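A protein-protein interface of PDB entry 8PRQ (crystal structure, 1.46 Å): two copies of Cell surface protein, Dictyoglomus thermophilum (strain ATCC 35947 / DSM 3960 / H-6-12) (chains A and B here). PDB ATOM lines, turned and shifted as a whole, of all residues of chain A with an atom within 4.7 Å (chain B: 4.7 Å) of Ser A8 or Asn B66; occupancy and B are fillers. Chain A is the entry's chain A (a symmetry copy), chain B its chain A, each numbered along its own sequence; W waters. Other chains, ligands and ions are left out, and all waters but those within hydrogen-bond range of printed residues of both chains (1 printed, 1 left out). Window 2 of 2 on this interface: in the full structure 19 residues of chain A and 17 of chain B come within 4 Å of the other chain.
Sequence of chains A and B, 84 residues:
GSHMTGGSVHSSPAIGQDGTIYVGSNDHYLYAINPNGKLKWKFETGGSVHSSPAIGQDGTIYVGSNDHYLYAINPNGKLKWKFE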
ATOM      1  N   GLY A   7       2.869  23.056  -4.080  1.00  0.00           N
ATOM      2  CA  GLY A   7       2.360  24.286  -3.509  1.00  0.00           C
ATOM      3  C   GLY A   7       3.475  25.017  -2.802  1.00  0.00           C
ATOM      4  O   GLY A   7       4.623  24.577  -2.806  1.00  0.00           O
ATOM      5  N   SER A   8       3.126  26.140  -2.171  1.00  0.00           N
ATOM      6  CA  SER A   8       4.153  26.960  -1.540  1.00  0.00           C
ATOM      7  C   SER A   8       4.931  26.179  -0.502  1.00  0.00           C
ATOM      8  O   SER A   8       4.368  25.400   0.266  1.00  0.00           O
ATOM      9  CB  SER A   8       3.516  28.127  -0.811  1.00  0.00           C
ATOM     10  OG  SER A   8       2.956  28.995  -1.744  1.00  0.00           O
ATOM     11  N   VAL A   9       6.232  26.428  -0.440  1.00  0.00           N
ATOM     12  CA  VAL A   9       7.075  25.827   0.588  1.00  0.00           C
ATOM     13  C   VAL A   9       7.249  26.905   1.651  1.00  0.00           C
ATOM     14  O   VAL A   9       8.178  27.708   1.595  1.00  0.00           O
ATOM     15  CB  VAL A   9       8.413  25.344   0.019  1.00  0.00           C
ATOM     16  CG1 VAL A   9       9.243  24.709   1.132  1.00  0.00           C
ATOM     17  CG2 VAL A   9       8.183  24.352  -1.123  1.00  0.00           C
ATOM     18  N   HIS A  10       6.340  26.940   2.632  1.00  0.00           N
ATOM     19  CA  HIS A  10       6.509  27.868   3.736  1.00  0.00           C
ATOM     20  C   HIS A  10       7.383  27.263   4.821  1.00  0.00           C
ATOM     21  O   HIS A  10       8.043  28.007   5.562  1.00  0.00           O
ATOM     22  CB  HIS A  10       5.180  28.190   4.426  1.00  0.00           C
ATOM     23  CG  HIS A  10       4.370  29.255   3.748  1.00  0.00           C
ATOM     24  ND1 HIS A  10       3.742  29.058   2.535  1.00  0.00           N
ATOM     25  CD2 HIS A  10       4.057  30.513   4.134  1.00  0.00           C
ATOM     26  CE1 HIS A  10       3.086  30.155   2.199  1.00  0.00           C
ATOM     27  NE2 HIS A  10       3.265  31.054   3.149  1.00  0.00           N
ATOM     28  N   SER A  25       5.386  21.170   2.659  1.00  0.00           N
ATOM     29  CA  SER A  25       4.808  21.917   1.561  1.00  0.00           C
ATOM     30  C   SER A  25       3.327  22.126   1.835  1.00  0.00           C
ATOM     31  O   SER A  25       2.680  21.323   2.514  1.00  0.00           O
ATOM     32  CB  SER A  25       4.968  21.206   0.200  1.00  0.00           C
ATOM     33  OG  SER A  25       4.271  21.936  -0.839  1.00  0.00           O
ATOM     34  N   ASN A  26       2.802  23.224   1.301  1.00  0.00           N
ATOM     35  CA  ASN A  26       1.370  23.486   1.377  1.00  0.00           C
ATOM     36  C   ASN A  26       0.568  22.495   0.546  1.00  0.00           C
ATOM     37  O   ASN A  26      -0.677  22.461   0.655  1.00  0.00           O
ATOM     38  CB  ASN A  26       1.118  24.927   0.945  1.00  0.00           C
ATOM     39  CG  ASN A  26       1.466  25.957   2.039  1.00  0.00           C
ATOM     40  OD1 ASN A  26       2.083  25.634   3.065  1.00  0.00           O
ATOM     41  ND2 ASN A  26       1.060  27.203   1.813  1.00  0.00           N
ATOM     42  N   GLY B  47       8.693  33.797  -6.113  1.00  0.00           N
ATOM     43  CA  GLY B  47       7.660  34.230  -5.191  1.00  0.00           C
ATOM     44  C   GLY B  47       8.290  34.508  -3.847  1.00  0.00           C
ATOM     45  O   GLY B  47       9.482  34.290  -3.658  1.00  0.00           O
ATOM     46  N   SER B  48       7.483  35.002  -2.904  1.00  0.00           N
ATOM     47  CA  SER B  48       8.005  35.350  -1.580  1.00  0.00           C
ATOM     48  C   SER B  48       8.774  34.196  -0.949  1.00  0.00           C
ATOM     49  O   SER B  48       8.390  33.034  -1.053  1.00  0.00           O
ATOM     50  CB  SER B  48       6.858  35.744  -0.653  1.00  0.00           C
ATOM     51  OG  SER B  48       6.264  36.944  -1.110  1.00  0.00           O
ATOM     52  N   HIS B  50       9.254  32.963   2.326  1.00  0.00           N
ATOM     53  CA  HIS B  50       8.842  32.941   3.726  1.00  0.00           C
ATOM     54  C   HIS B  50       9.657  31.923   4.509  1.00  0.00           C
ATOM     55  O   HIS B  50       9.934  32.123   5.702  1.00  0.00           O
ATOM     56  CB  HIS B  50       7.362  32.537   3.834  1.00  0.00           C
ATOM     57  CG  HIS B  50       6.394  33.668   3.651  1.00  0.00           C
ATOM     58  ND1 HIS B  50       5.411  33.654   2.686  1.00  0.00           N
ATOM     59  CD2 HIS B  50       6.237  34.829   4.329  1.00  0.00           C
ATOM     60  CE1 HIS B  50       4.706  34.769   2.761  1.00  0.00           C
ATOM     61  NE2 HIS B  50       5.186  35.497   3.750  1.00  0.00           N
ATOM     62  N   GLY B  64      12.924  27.214   0.932  1.00  0.00           N
ATOM     63  CA  GLY B  64      11.725  27.158   0.113  1.00  0.00           C
ATOM     64  C   GLY B  64      11.249  28.512  -0.367  1.00  0.00           C
ATOM     65  O   GLY B  64      11.650  29.577   0.106  1.00  0.00           O
ATOM     66  N   SER B  65      10.333  28.465  -1.328  1.00  0.00           N
ATOM     67  CA  SER B  65       9.761  29.671  -1.894  1.00  0.00           C
ATOM     68  C   SER B  65       8.280  29.421  -2.118  1.00  0.00           C
ATOM     69  O   SER B  65       7.857  28.280  -2.295  1.00  0.00           O
ATOM     70  CB  SER B  65      10.435  30.020  -3.232  1.00  0.00           C
ATOM     71  OG  SER B  65       9.751  31.089  -3.891  1.00  0.00           O
ATOM     72  N   ASN B  66       7.483  30.502  -2.077  1.00  0.00           N
ATOM     73  CA  ASN B  66       6.073  30.399  -2.425  1.00  0.00           C
ATOM     74  C   ASN B  66       5.861  30.069  -3.891  1.00  0.00           C
ATOM     75  O   ASN B  66       4.702  29.834  -4.299  1.00  0.00           O
ATOM     76  CB  ASN B  66       5.389  31.705  -2.043  1.00  0.00           C
ATOM     77  CG  ASN B  66       5.171  31.843  -0.543  1.00  0.00           C
ATOM     78  OD1 ASN B  66       5.613  31.007   0.256  1.00  0.00           O
ATOM     79  ND2 ASN B  66       4.515  32.924  -0.152  1.00  0.00           N
ATOM     80  N   ASP B  67       6.932  30.012  -4.683  1.00  0.00           N
ATOM     81  CA  ASP B  67       6.838  29.564  -6.071  1.00  0.00           C
ATOM     82  C   ASP B  67       6.752  28.049  -6.193  1.00  0.00           C
ATOM     83  O   ASP B  67       6.670  27.543  -7.316  1.00  0.00           O
ATOM     84  CB  ASP B  67       7.962  30.154  -6.922  1.00  0.00           C
ATOM     85  CG  ASP B  67       9.306  29.526  -6.671  1.00  0.00           C
ATOM     86  OD1 ASP B  67       9.424  28.552  -5.891  1.00  0.00           O
ATOM     87  OD2 ASP B  67      10.263  30.031  -7.292  1.00  0.00           O
ATOM     88  N   HIS B  68       6.694  27.339  -5.068  1.00  0.00           N
ATOM     89  CA  HIS B  68       6.547  25.884  -4.920  1.00  0.00           C
ATOM     90  C   HIS B  68       7.855  25.119  -4.880  1.00  0.00           C
ATOM     91  O   HIS B  68       7.810  23.913  -4.679  1.00  0.00           O
ATOM     92  CB  HIS B  68       5.636  25.238  -5.977  1.00  0.00           C
ATOM     93  CG  HIS B  68       4.285  25.845  -6.021  1.00  0.00           C
ATOM     94  ND1 HIS B  68       3.247  25.369  -6.793  1.00  0.00           N
ATOM     95  CD2 HIS B  68       3.815  26.925  -5.371  1.00  0.00           C
ATOM     96  CE1 HIS B  68       2.187  26.138  -6.608  1.00  0.00           C
ATOM     97  NE2 HIS B  68       2.505  27.084  -5.738  1.00  0.00           N
HETATM   98  O   HOH W   1       1.559  30.695  -4.397  1.00  0.00           O
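Water W1 lies within hydrogen-bond range of the backbone carbonyl oxygen (O) of Asn B66 (3.3 Å) and the side-chain hydroxyl (OG) of Ser A8 (3.4 Å).
The side-chain hydroxyl of Ser B65 is in hydrogen-bond range of the backbone carbonyl oxygen of Gly B47 (3.2 Å).
The backbone NH (N) of Asn B66 is in hydrogen-bond range of the backbone carbonyl oxygen (O) of Ser B48.
A ring nitrogen (ND1) of His B50 is in hydrogen-bond range of the side-chain amide nitrogen of Asn B66 (3.1 Å).
The backbone NH (N) of Asp B67 lies close to the side-chain hydroxyl (OG) of Ser B65 (3.1 Å).
O of Gly A7 lies within hydrogen-bond range of OG of Ser A25 (3.3 Å).
N of Asn A26 lies within hydrogen-bond range of O of Ser A8.
Among the printed residues, merely in contact across the chains: Gly A7 with His B68 (3.1 Å), Ser A8 with His B68 (3.4 Å), Val A9 with Gly B64 (3.6 Å), Val A9 with His B68 (3.6 Å) and His A10 with Asn B66 (3.3 Å).
Hydrophobic or aromatic side chains of chain A that line the printed part of chain B: Val A9 and His A10.
Printed residues of chain B that touch a printed residue of chain A: His B50, Gly B64, Ser B65, Asn B66 and His B68.
Among the printed residues, 8 pairs touch across the chains.
Among the printed residues, no Asp or Glu carboxylate lies within 4 Å of a Lys or Arg side-chain nitrogen of the other chain.
No position is printed for both chains.
Of the 8 pairs that touch across the chains among the printed residues, none has its exchanged pair printed and touching as well.
ND1 of His B50 lies within hydrogen-bond range of NE2 of His A10, at 3.4 Å.
The backbone NH of Val A9 lies within hydrogen-bond range of the backbone carbonyl oxygen of Ser B65 (3.1 Å).
The backbone carbonyl oxygen (O) of Asn B66 lies within hydrogen-bond range of the side-chain hydroxyl (OG) of Ser A8 (3.2 Å).
Printed residues of chain B within 4 Å of Ser A8: Asn B66 and His B68.
Of the printed residues of chain A, His B50 touches His A10.
Of the printed residues of chain A, His B68 touches Gly A7 (3.1 Å), Ser A8 (3.4 Å) and Val A9 (3.6 Å).
Of the printed residues of chain B, Gly A7 touches His B68 (3.1 Å).
The nearest printed residue of chain A that does not touch Asn B66 is Val A9 (4.4 Å).
The nearest printed residue of chain B that does not touch His A10 is Ser B65 (5.3 Å).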
